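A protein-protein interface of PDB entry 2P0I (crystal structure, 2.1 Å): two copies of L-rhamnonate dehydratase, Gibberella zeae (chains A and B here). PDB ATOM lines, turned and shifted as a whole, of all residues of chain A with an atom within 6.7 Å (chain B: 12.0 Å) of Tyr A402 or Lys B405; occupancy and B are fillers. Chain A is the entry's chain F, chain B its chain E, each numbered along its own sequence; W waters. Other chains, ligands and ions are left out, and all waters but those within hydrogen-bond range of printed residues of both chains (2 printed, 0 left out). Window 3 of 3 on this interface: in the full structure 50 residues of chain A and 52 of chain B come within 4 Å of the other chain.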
ATOM      1  N   ILE A  18      37.565  14.637   5.638  1.00  0.00           N
ATOM      2  CA  ILE A  18      36.761  13.449   5.402  1.00  0.00           C
ATOM      3  C   ILE A  18      37.657  12.299   4.950  1.00  0.00           C
ATOM      4  O   ILE A  18      38.304  12.378   3.908  1.00  0.00           O
ATOM      5  CB  ILE A  18      35.623  13.715   4.374  1.00  0.00           C
ATOM      6  CG1 ILE A  18      34.697  14.827   4.877  1.00  0.00           C
ATOM      7  CG2 ILE A  18      34.795  12.460   4.138  1.00  0.00           C
ATOM      8  CD1 ILE A  18      34.867  16.139   4.163  1.00  0.00           C
ATOM      9  N   PRO A  87      31.095  13.980   6.166  1.00  0.00           N
ATOM     10  CA  PRO A  87      30.759  15.311   5.649  1.00  0.00           C
ATOM     11  C   PRO A  87      29.834  16.208   6.495  1.00  0.00           C
ATOM     12  O   PRO A  87      30.211  17.352   6.739  1.00  0.00           O
ATOM     13  CB  PRO A  87      30.205  15.027   4.250  1.00  0.00           C
ATOM     14  CG  PRO A  87      30.869  13.745   3.851  1.00  0.00           C
ATOM     15  CD  PRO A  87      30.942  12.943   5.126  1.00  0.00           C
ATOM     16  N   ILE A 398      40.405  14.154   2.781  1.00  0.00           N
ATOM     17  CA  ILE A 398      39.926  15.193   1.886  1.00  0.00           C
ATOM     18  C   ILE A 398      39.471  16.377   2.738  1.00  0.00           C
ATOM     19  O   ILE A 398      38.611  16.208   3.604  1.00  0.00           O
ATOM     20  CB  ILE A 398      38.711  14.673   1.075  1.00  0.00           C
ATOM     21  CG1 ILE A 398      39.016  13.299   0.466  1.00  0.00           C
ATOM     22  CG2 ILE A 398      38.293  15.684   0.006  1.00  0.00           C
ATOM     23  CD1 ILE A 398      37.835  12.349   0.461  1.00  0.00           C
ATOM     24  N   PRO A 399      40.038  17.580   2.496  1.00  0.00           N
ATOM     25  CA  PRO A 399      39.650  18.758   3.279  1.00  0.00           C
ATOM     26  C   PRO A 399      38.171  19.087   3.111  1.00  0.00           C
ATOM     27  O   PRO A 399      37.580  18.793   2.070  1.00  0.00           O
ATOM     28  CB  PRO A 399      40.507  19.887   2.682  1.00  0.00           C
ATOM     29  CG  PRO A 399      41.625  19.209   1.994  1.00  0.00           C
ATOM     30  CD  PRO A 399      41.061  17.910   1.489  1.00  0.00           C
ATOM     31  N   SER A 400      37.587  19.698   4.133  1.00  0.00           N
ATOM     32  CA  SER A 400      36.140  19.881   4.199  1.00  0.00           C
ATOM     33  C   SER A 400      35.649  21.094   3.398  1.00  0.00           C
ATOM     34  O   SER A 400      34.448  21.377   3.373  1.00  0.00           O
ATOM     35  CB  SER A 400      35.693  19.987   5.658  1.00  0.00           C
ATOM     36  OG  SER A 400      36.574  20.812   6.407  1.00  0.00           O
ATOM     37  N   ASP A 401      36.585  21.784   2.739  1.00  0.00           N
ATOM     38  CA  ASP A 401      36.357  23.084   2.093  1.00  0.00           C
ATOM     39  C   ASP A 401      35.195  23.073   1.110  1.00  0.00           C
ATOM     40  O   ASP A 401      34.415  24.032   1.055  1.00  0.00           O
ATOM     41  CB  ASP A 401      37.626  23.551   1.370  1.00  0.00           C
ATOM     42  CG  ASP A 401      38.823  23.682   2.301  1.00  0.00           C
ATOM     43  OD1 ASP A 401      38.663  23.500   3.530  1.00  0.00           O
ATOM     44  OD2 ASP A 401      39.928  23.972   1.795  1.00  0.00           O
ATOM     45  N   TYR A 402      35.081  21.969   0.364  1.00  0.00           N
ATOM     46  CA  TYR A 402      34.108  21.812  -0.717  1.00  0.00           C
ATOM     47  C   TYR A 402      32.652  21.887  -0.241  1.00  0.00           C
ATOM     48  O   TYR A 402      31.767  22.293  -1.001  1.00  0.00           O
ATOM     49  CB  TYR A 402      34.367  20.511  -1.499  1.00  0.00           C
ATOM     50  CG  TYR A 402      33.838  19.243  -0.837  1.00  0.00           C
ATOM     51  CD1 TYR A 402      32.644  18.646  -1.266  1.00  0.00           C
ATOM     52  CD2 TYR A 402      34.531  18.641   0.216  1.00  0.00           C
ATOM     53  CE1 TYR A 402      32.155  17.484  -0.657  1.00  0.00           C
ATOM     54  CE2 TYR A 402      34.050  17.480   0.826  1.00  0.00           C
ATOM     55  CZ  TYR A 402      32.865  16.908   0.387  1.00  0.00           C
ATOM     56  OH  TYR A 402      32.399  15.765   0.992  1.00  0.00           O
ATOM     57  N   LEU A 403      32.423  21.503   1.018  1.00  0.00           N
ATOM     58  CA  LEU A 403      31.100  21.569   1.653  1.00  0.00           C
ATOM     59  C   LEU A 403      30.638  23.008   1.908  1.00  0.00           C
ATOM     60  O   LEU A 403      29.451  23.251   2.134  1.00  0.00           O
ATOM     61  CB  LEU A 403      31.080  20.760   2.961  1.00  0.00           C
ATOM     62  CG  LEU A 403      31.386  19.254   2.877  1.00  0.00           C
ATOM     63  CD1 LEU A 403      31.888  18.721   4.211  1.00  0.00           C
ATOM     64  CD2 LEU A 403      30.185  18.447   2.392  1.00  0.00           C
ATOM     65  N   PHE A 404      31.580  23.949   1.854  1.00  0.00           N
ATOM     66  CA  PHE A 404      31.296  25.369   2.051  1.00  0.00           C
ATOM     67  C   PHE A 404      31.402  26.184   0.757  1.00  0.00           C
ATOM     68  O   PHE A 404      31.211  27.405   0.773  1.00  0.00           O
ATOM     69  CB  PHE A 404      32.210  25.955   3.130  1.00  0.00           C
ATOM     70  CG  PHE A 404      32.308  25.110   4.371  1.00  0.00           C
ATOM     71  CD1 PHE A 404      31.299  25.136   5.328  1.00  0.00           C
ATOM     72  CD2 PHE A 404      33.415  24.291   4.585  1.00  0.00           C
ATOM     73  CE1 PHE A 404      31.391  24.360   6.474  1.00  0.00           C
ATOM     74  CE2 PHE A 404      33.511  23.511   5.730  1.00  0.00           C
ATOM     75  CZ  PHE A 404      32.500  23.546   6.674  1.00  0.00           C
ATOM     76  N   LYS A 405      31.694  25.506  -0.354  1.00  0.00           N
ATOM     77  CA  LYS A 405      31.709  26.132  -1.682  1.00  0.00           C
ATOM     78  C   LYS A 405      30.312  26.201  -2.309  1.00  0.00           C
ATOM     79  O   LYS A 405      30.005  25.481  -3.263  1.00  0.00           O
ATOM     80  CB  LYS A 405      32.689  25.413  -2.619  1.00  0.00           C
ATOM     81  CG  LYS A 405      34.010  26.143  -2.834  1.00  0.00           C
ATOM     82  CD  LYS A 405      35.158  25.445  -2.119  1.00  0.00           C
ATOM     83  CE  LYS A 405      36.281  26.418  -1.791  1.00  0.00           C
ATOM     84  NZ  LYS A 405      37.232  26.573  -2.924  1.00  0.00           N
ATOM     85  N   VAL A 406      29.476  27.082  -1.767  1.00  0.00           N
ATOM     86  CA  VAL A 406      28.084  27.202  -2.194  1.00  0.00           C
ATOM     87  C   VAL A 406      27.943  28.223  -3.339  1.00  0.00           C
ATOM     88  O   VAL A 406      28.385  29.367  -3.207  1.00  0.00           O
ATOM     89  CB  VAL A 406      27.125  27.485  -0.981  1.00  0.00           C
ATOM     90  CG1 VAL A 406      27.669  28.585  -0.061  1.00  0.00           C
ATOM     91  CG2 VAL A 406      25.704  27.795  -1.435  1.00  0.00           C
ATOM     92  N   SER B  16      16.306  17.845  -3.256  1.00  0.00           N
ATOM     93  CA  SER B  16      16.480  18.782  -2.146  1.00  0.00           C
ATOM     94  C   SER B  16      17.198  20.075  -2.534  1.00  0.00           C
ATOM     95  O   SER B  16      18.044  20.086  -3.432  1.00  0.00           O
ATOM     96  CB  SER B  16      17.139  18.110  -0.933  1.00  0.00           C
ATOM     97  OG  SER B  16      18.496  17.792  -1.179  1.00  0.00           O
ATOM     98  N   ILE B  18      18.799  23.902  -0.834  1.00  0.00           N
ATOM     99  CA  ILE B  18      19.103  24.881   0.211  1.00  0.00           C
ATOM    100  C   ILE B  18      18.471  26.220  -0.179  1.00  0.00           C
ATOM    101  O   ILE B  18      18.514  26.615  -1.343  1.00  0.00           O
ATOM    102  CB  ILE B  18      20.646  25.013   0.445  1.00  0.00           C
ATOM    103  CG1 ILE B  18      21.229  23.693   0.957  1.00  0.00           C
ATOM    104  CG2 ILE B  18      20.981  26.096   1.467  1.00  0.00           C
ATOM    105  CD1 ILE B  18      22.073  22.968  -0.050  1.00  0.00           C
ATOM    106  N   PRO B  87      22.184  22.540   4.640  1.00  0.00           N
ATOM    107  CA  PRO B  87      23.148  21.626   4.018  1.00  0.00           C
ATOM    108  C   PRO B  87      23.315  20.210   4.613  1.00  0.00           C
ATOM    109  O   PRO B  87      23.209  19.246   3.851  1.00  0.00           O
ATOM    110  CB  PRO B  87      24.456  22.426   4.025  1.00  0.00           C
ATOM    111  CG  PRO B  87      24.017  23.845   4.054  1.00  0.00           C
ATOM    112  CD  PRO B  87      22.791  23.856   4.916  1.00  0.00           C
ATOM    113  N   PRO B  88      23.561  20.064   5.942  1.00  0.00           N
ATOM    114  CA  PRO B  88      23.732  18.677   6.411  1.00  0.00           C
ATOM    115  C   PRO B  88      22.441  17.836   6.392  1.00  0.00           C
ATOM    116  O   PRO B  88      22.507  16.606   6.307  1.00  0.00           O
ATOM    117  CB  PRO B  88      24.231  18.858   7.847  1.00  0.00           C
ATOM    118  CG  PRO B  88      23.659  20.160   8.280  1.00  0.00           C
ATOM    119  CD  PRO B  88      23.701  21.024   7.060  1.00  0.00           C
ATOM    120  N   CYS B  90      20.104  18.207   3.811  1.00  0.00           N
ATOM    121  CA  CYS B  90      20.129  17.834   2.388  1.00  0.00           C
ATOM    122  C   CYS B  90      21.082  16.692   2.071  1.00  0.00           C
ATOM    123  O   CYS B  90      20.805  15.875   1.190  1.00  0.00           O
ATOM    124  CB  CYS B  90      20.549  19.028   1.537  1.00  0.00           C
ATOM    125  SG  CYS B  90      19.371  20.373   1.450  1.00  0.00           S
ATOM    126  N   TRP B  91      22.217  16.670   2.767  1.00  0.00           N
ATOM    127  CA  TRP B  91      23.192  15.597   2.631  1.00  0.00           C
ATOM    128  C   TRP B  91      22.553  14.266   2.991  1.00  0.00           C
ATOM    129  O   TRP B  91      22.631  13.309   2.216  1.00  0.00           O
ATOM    130  CB  TRP B  91      24.416  15.857   3.513  1.00  0.00           C
ATOM    131  CG  TRP B  91      25.584  14.980   3.177  1.00  0.00           C
ATOM    132  CD1 TRP B  91      26.557  15.233   2.257  1.00  0.00           C
ATOM    133  CD2 TRP B  91      25.902  13.707   3.759  1.00  0.00           C
ATOM    134  NE1 TRP B  91      27.462  14.201   2.225  1.00  0.00           N
ATOM    135  CE2 TRP B  91      27.089  13.252   3.142  1.00  0.00           C
ATOM    136  CE3 TRP B  91      25.302  12.908   4.746  1.00  0.00           C
ATOM    137  CZ2 TRP B  91      27.689  12.028   3.473  1.00  0.00           C
ATOM    138  CZ3 TRP B  91      25.899  11.688   5.077  1.00  0.00           C
ATOM    139  CH2 TRP B  91      27.083  11.264   4.442  1.00  0.00           C
ATOM    140  N   LEU B  92      21.891  14.239   4.149  1.00  0.00           N
ATOM    141  CA  LEU B  92      21.289  13.020   4.691  1.00  0.00           C
ATOM    142  C   LEU B  92      20.105  12.504   3.874  1.00  0.00           C
ATOM    143  O   LEU B  92      19.913  11.292   3.800  1.00  0.00           O
ATOM    144  CB  LEU B  92      20.904  13.194   6.170  1.00  0.00           C
ATOM    145  CG  LEU B  92      22.033  13.294   7.212  1.00  0.00           C
ATOM    146  CD1 LEU B  92      21.513  13.932   8.501  1.00  0.00           C
ATOM    147  CD2 LEU B  92      22.691  11.935   7.513  1.00  0.00           C
ATOM    148  N   HIS B  94      19.670  12.338   0.620  1.00  0.00           N
ATOM    149  CA  HIS B  94      20.078  11.549  -0.537  1.00  0.00           C
ATOM    150  C   HIS B  94      20.990  10.397  -0.159  1.00  0.00           C
ATOM    151  O   HIS B  94      20.931   9.329  -0.765  1.00  0.00           O
ATOM    152  CB  HIS B  94      20.747  12.445  -1.568  1.00  0.00           C
ATOM    153  CG  HIS B  94      19.875  13.567  -2.022  1.00  0.00           C
ATOM    154  ND1 HIS B  94      18.854  13.390  -2.934  1.00  0.00           N
ATOM    155  CD2 HIS B  94      19.838  14.871  -1.662  1.00  0.00           C
ATOM    156  CE1 HIS B  94      18.237  14.542  -3.127  1.00  0.00           C
ATOM    157  NE2 HIS B  94      18.817  15.458  -2.370  1.00  0.00           N
ATOM    158  N   GLN B  95      21.840  10.626   0.840  1.00  0.00           N
ATOM    159  CA  GLN B  95      22.782   9.611   1.281  1.00  0.00           C
ATOM    160  C   GLN B  95      22.064   8.506   2.036  1.00  0.00           C
ATOM    161  O   GLN B  95      22.359   7.321   1.835  1.00  0.00           O
ATOM    162  CB  GLN B  95      23.895  10.217   2.142  1.00  0.00           C
ATOM    163  CG  GLN B  95      24.884  11.089   1.369  1.00  0.00           C
ATOM    164  CD  GLN B  95      25.811  10.305   0.448  1.00  0.00           C
ATOM    165  OE1 GLN B  95      25.738  10.441  -0.771  1.00  0.00           O
ATOM    166  NE2 GLN B  95      26.691   9.489   1.028  1.00  0.00           N
ATOM    167  N   ILE B 398      19.124  26.864  -4.066  1.00  0.00           N
ATOM    168  CA  ILE B 398      20.370  26.235  -4.479  1.00  0.00           C
ATOM    169  C   ILE B 398      20.183  24.720  -4.421  1.00  0.00           C
ATOM    170  O   ILE B 398      19.893  24.181  -3.353  1.00  0.00           O
ATOM    171  CB  ILE B 398      21.533  26.657  -3.538  1.00  0.00           C
ATOM    172  CG1 ILE B 398      21.742  28.175  -3.593  1.00  0.00           C
ATOM    173  CG2 ILE B 398      22.821  25.908  -3.881  1.00  0.00           C
ATOM    174  CD1 ILE B 398      22.065  28.816  -2.251  1.00  0.00           C
ATOM    175  N   PRO B 399      20.344  24.029  -5.567  1.00  0.00           N
ATOM    176  CA  PRO B 399      20.374  22.564  -5.586  1.00  0.00           C
ATOM    177  C   PRO B 399      21.512  22.001  -4.739  1.00  0.00           C
ATOM    178  O   PRO B 399      22.591  22.594  -4.669  1.00  0.00           O
ATOM    179  CB  PRO B 399      20.604  22.237  -7.065  1.00  0.00           C
ATOM    180  CG  PRO B 399      20.110  23.439  -7.795  1.00  0.00           C
ATOM    181  CD  PRO B 399      20.498  24.588  -6.921  1.00  0.00           C
ATOM    182  N   SER B 400      21.264  20.860  -4.105  1.00  0.00           N
ATOM    183  CA  SER B 400      22.156  20.351  -3.069  1.00  0.00           C
ATOM    184  C   SER B 400      23.333  19.557  -3.634  1.00  0.00           C
ATOM    185  O   SER B 400      24.111  18.970  -2.870  1.00  0.00           O
ATOM    186  CB  SER B 400      21.374  19.513  -2.054  1.00  0.00           C
ATOM    187  OG  SER B 400      20.763  18.398  -2.673  1.00  0.00           O
ATOM    188  N   ASP B 401      23.470  19.567  -4.964  1.00  0.00           N
ATOM    189  CA  ASP B 401      24.391  18.687  -5.695  1.00  0.00           C
ATOM    190  C   ASP B 401      25.863  18.906  -5.344  1.00  0.00           C
ATOM    191  O   ASP B 401      26.661  17.962  -5.392  1.00  0.00           O
ATOM    192  CB  ASP B 401      24.192  18.829  -7.210  1.00  0.00           C
ATOM    193  CG  ASP B 401      22.748  18.607  -7.641  1.00  0.00           C
ATOM    194  OD1 ASP B 401      21.971  17.999  -6.877  1.00  0.00           O
ATOM    195  OD2 ASP B 401      22.389  19.044  -8.755  1.00  0.00           O
ATOM    196  N   TYR B 402      26.202  20.145  -4.974  1.00  0.00           N
ATOM    197  CA  TYR B 402      27.572  20.535  -4.630  1.00  0.00           C
ATOM    198  C   TYR B 402      28.153  19.819  -3.410  1.00  0.00           C
ATOM    199  O   TYR B 402      29.370  19.654  -3.305  1.00  0.00           O
ATOM    200  CB  TYR B 402      27.688  22.059  -4.474  1.00  0.00           C
ATOM    201  CG  TYR B 402      27.151  22.635  -3.176  1.00  0.00           C
ATOM    202  CD1 TYR B 402      28.004  22.898  -2.100  1.00  0.00           C
ATOM    203  CD2 TYR B 402      25.801  22.951  -3.036  1.00  0.00           C
ATOM    204  CE1 TYR B 402      27.522  23.437  -0.909  1.00  0.00           C
ATOM    205  CE2 TYR B 402      25.310  23.492  -1.851  1.00  0.00           C
ATOM    206  CZ  TYR B 402      26.176  23.732  -0.793  1.00  0.00           C
ATOM    207  OH  TYR B 402      25.700  24.267   0.383  1.00  0.00           O
ATOM    208  N   LEU B 403      27.277  19.398  -2.501  1.00  0.00           N
ATOM    209  CA  LEU B 403      27.674  18.709  -1.276  1.00  0.00           C
ATOM    210  C   LEU B 403      28.137  17.271  -1.536  1.00  0.00           C
ATOM    211  O   LEU B 403      28.781  16.657  -0.677  1.00  0.00           O
ATOM    212  CB  LEU B 403      26.529  18.733  -0.260  1.00  0.00           C
ATOM    213  CG  LEU B 403      26.159  20.108   0.304  1.00  0.00           C
ATOM    214  CD1 LEU B 403      24.712  20.136   0.775  1.00  0.00           C
ATOM    215  CD2 LEU B 403      27.110  20.528   1.424  1.00  0.00           C
ATOM    216  N   PHE B 404      27.813  16.752  -2.722  1.00  0.00           N
ATOM    217  CA  PHE B 404      28.202  15.401  -3.142  1.00  0.00           C
ATOM    218  C   PHE B 404      29.229  15.413  -4.274  1.00  0.00           C
ATOM    219  O   PHE B 404      29.366  14.435  -5.012  1.00  0.00           O
ATOM    220  CB  PHE B 404      26.968  14.597  -3.569  1.00  0.00           C
ATOM    221  CG  PHE B 404      25.791  14.755  -2.651  1.00  0.00           C
ATOM    222  CD1 PHE B 404      25.734  14.064  -1.442  1.00  0.00           C
ATOM    223  CD2 PHE B 404      24.735  15.591  -2.997  1.00  0.00           C
ATOM    224  CE1 PHE B 404      24.643  14.208  -0.595  1.00  0.00           C
ATOM    225  CE2 PHE B 404      23.642  15.745  -2.156  1.00  0.00           C
ATOM    226  CZ  PHE B 404      23.594  15.047  -0.955  1.00  0.00           C
ATOM    227  N   LYS B 405      29.945  16.526  -4.410  1.00  0.00           N
ATOM    228  CA  LYS B 405      31.048  16.625  -5.362  1.00  0.00           C
ATOM    229  C   LYS B 405      32.394  16.554  -4.648  1.00  0.00           C
ATOM    230  O   LYS B 405      33.030  17.577  -4.377  1.00  0.00           O
ATOM    231  CB  LYS B 405      30.930  17.896  -6.209  1.00  0.00           C
ATOM    232  CG  LYS B 405      30.521  17.641  -7.651  1.00  0.00           C
ATOM    233  CD  LYS B 405      29.036  17.874  -7.866  1.00  0.00           C
ATOM    234  CE  LYS B 405      28.650  17.620  -9.314  1.00  0.00           C
ATOM    235  NZ  LYS B 405      27.446  18.398  -9.715  1.00  0.00           N
ATOM    236  N   VAL B 406      32.814  15.327  -4.345  1.00  0.00           N
ATOM    237  CA  VAL B 406      34.013  15.078  -3.548  1.00  0.00           C
ATOM    238  C   VAL B 406      35.262  14.935  -4.435  1.00  0.00           C
ATOM    239  O   VAL B 406      35.312  14.060  -5.303  1.00  0.00           O
ATOM    240  CB  VAL B 406      33.818  13.870  -2.559  1.00  0.00           C
ATOM    241  CG1 VAL B 406      33.109  12.679  -3.227  1.00  0.00           C
ATOM    242  CG2 VAL B 406      35.133  13.447  -1.918  1.00  0.00           C
ATOM    243  N   PRO B 407      36.262  15.818  -4.240  1.00  0.00           N
ATOM    244  CA  PRO B 407      37.540  15.717  -4.956  1.00  0.00           C
ATOM    245  C   PRO B 407      38.405  14.537  -4.493  1.00  0.00           C
ATOM    246  O   PRO B 407      38.229  14.045  -3.375  1.00  0.00           O
ATOM    247  CB  PRO B 407      38.227  17.048  -4.636  1.00  0.00           C
ATOM    248  CG  PRO B 407      37.637  17.479  -3.341  1.00  0.00           C
ATOM    249  CD  PRO B 407      36.224  16.984  -3.336  1.00  0.00           C
ATOM    250  N   GLU B 408      39.328  14.097  -5.349  1.00  0.00           N
ATOM    251  CA  GLU B 408      40.098  12.870  -5.112  1.00  0.00           C
ATOM    252  C   GLU B 408      41.338  13.133  -4.260  1.00  0.00           C
ATOM    253  O   GLU B 408      42.068  12.205  -3.905  1.00  0.00           O
ATOM    254  CB  GLU B 408      40.502  12.210  -6.434  1.00  0.00           C
ATOM    255  CG  GLU B 408      39.334  11.729  -7.281  1.00  0.00           C
ATOM    256  CD  GLU B 408      38.977  12.711  -8.379  1.00  0.00           C
ATOM    257  OE1 GLU B 408      38.484  13.814  -8.059  1.00  0.00           O
ATOM    258  OE2 GLU B 408      39.192  12.381  -9.564  1.00  0.00           O
HETATM  259  O   HOH W   1      27.322  24.685   2.807  1.00  0.00           O
HETATM  260  O   HOH W   2      29.922  14.400   0.443  1.00  0.00           O
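The backbone NH (N) of Ile B18 sits at hydrogen-bond distance from the backbone carbonyl oxygen (O) of Ile B398. The backbone carbonyl oxygen (O) of Ile A398 sits at hydrogen-bond distance from the backbone NH (N) of Ile A18 (2.8 Å).
CB of Pro A87 touches NE1 of Trp B91, at 3.5 Å. Ile A398 touches Val B406 (CD1 to CG2, 3.8 Å). CG2 of Ile A398 touches O of Pro B407 (3.8 Å). Tyr B402 touches Tyr A402 (CD1 to O, 3.97 Å). Tyr A402 touches Lys B405 (CD1 to O, 3.3 Å). Leu A403 touches Tyr B402 (O to CE1, 3.6 Å). Leu A403 touches Leu B403 (O to CD2, 3.7 Å). Lys A405 touches Tyr B402 (O to CD1, 3.5 Å). Ile B398 touches Val A406. CB of Val A406 touches OH of Tyr B402 (3.8 Å).
No residue of chain B comes within 4 Å of Ile A18. Ile A398 touches just these residues of chain B: Val B406 and Pro B407. No residue of chain B comes within 4 Å of Pro A399. Ser A400 touches none of the printed residues of chain B. No residue of chain B comes within 4 Å of Asp A401. Printed residues of chain B within 4 Å of Tyr A402: Tyr B402, Leu B403 and Lys B405. Of chain B, only Tyr B402 and Leu B403 come within 4 Å of Leu A403. No residue of chain B comes within 4 Å of Phe A404. Of the printed residues of chain B, Lys A405 touches Tyr B402. Printed residues of chain B within 4 Å of Val A406: Ile B398 and Tyr B402. Ser B16 touches none of the printed residues of chain A. Of the printed residues of chain A, Trp B91 touches Pro A87. His B94 touches none of the printed residues of chain A. Printed residues of chain A within 4 Å of Ile B398: Val A406 (3.9 Å). Of the printed residues of chain A, Val B406 touches Ile A398. Of the printed residues of chain A, Pro B407 touches Ile A398 (3.8 Å). The nearest residue of chain B that does not touch Tyr A402 is Pro B407 (4.1 Å).
Of the 20 printed residues of chain B, 7 touch a printed residue of chain A. Of the 11 printed residues of chain A, 6 touch a printed residue of chain B. Hydrophobic or aromatic side chains of chain A within 4 Å of the printed part of chain B: Pro A87, Ile A398, Tyr A402, Leu A403 and Val A406. Among the printed residues, 11 pairs touch across the chains. Among the printed residues, no Asp or Glu carboxylate lies within 4 Å of a Lys or Arg side-chain nitrogen of the other chain.
Ile A398 touches Val B406, and with the chains exchanged Val A406 touches Ile B398. Tyr A402 touches its own counterpart, Tyr B402. Leu B403 touches its own counterpart, Leu A403. Val A406 touches Tyr B402, but with the chains exchanged Tyr A402 does not touch Val B406 (4.2 Å). Of the 11 pairs that touch across the chains among the printed residues, 8 have their exchanged pair printed and touching as well.
Water W1 bridges the backbone carbonyl oxygen (O) of Leu A403 (2.7 Å) and the side-chain hydroxyl (OH) of Tyr B402 (2.9 Å). Water W2 lies within hydrogen-bond range of the backbone carbonyl oxygen (O) of Leu B403 (2.8 Å), the side-chain hydroxyl (OH) of Tyr A402 (2.9 Å) and the indole nitrogen (NE1) of Trp B91 (3.0 Å).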
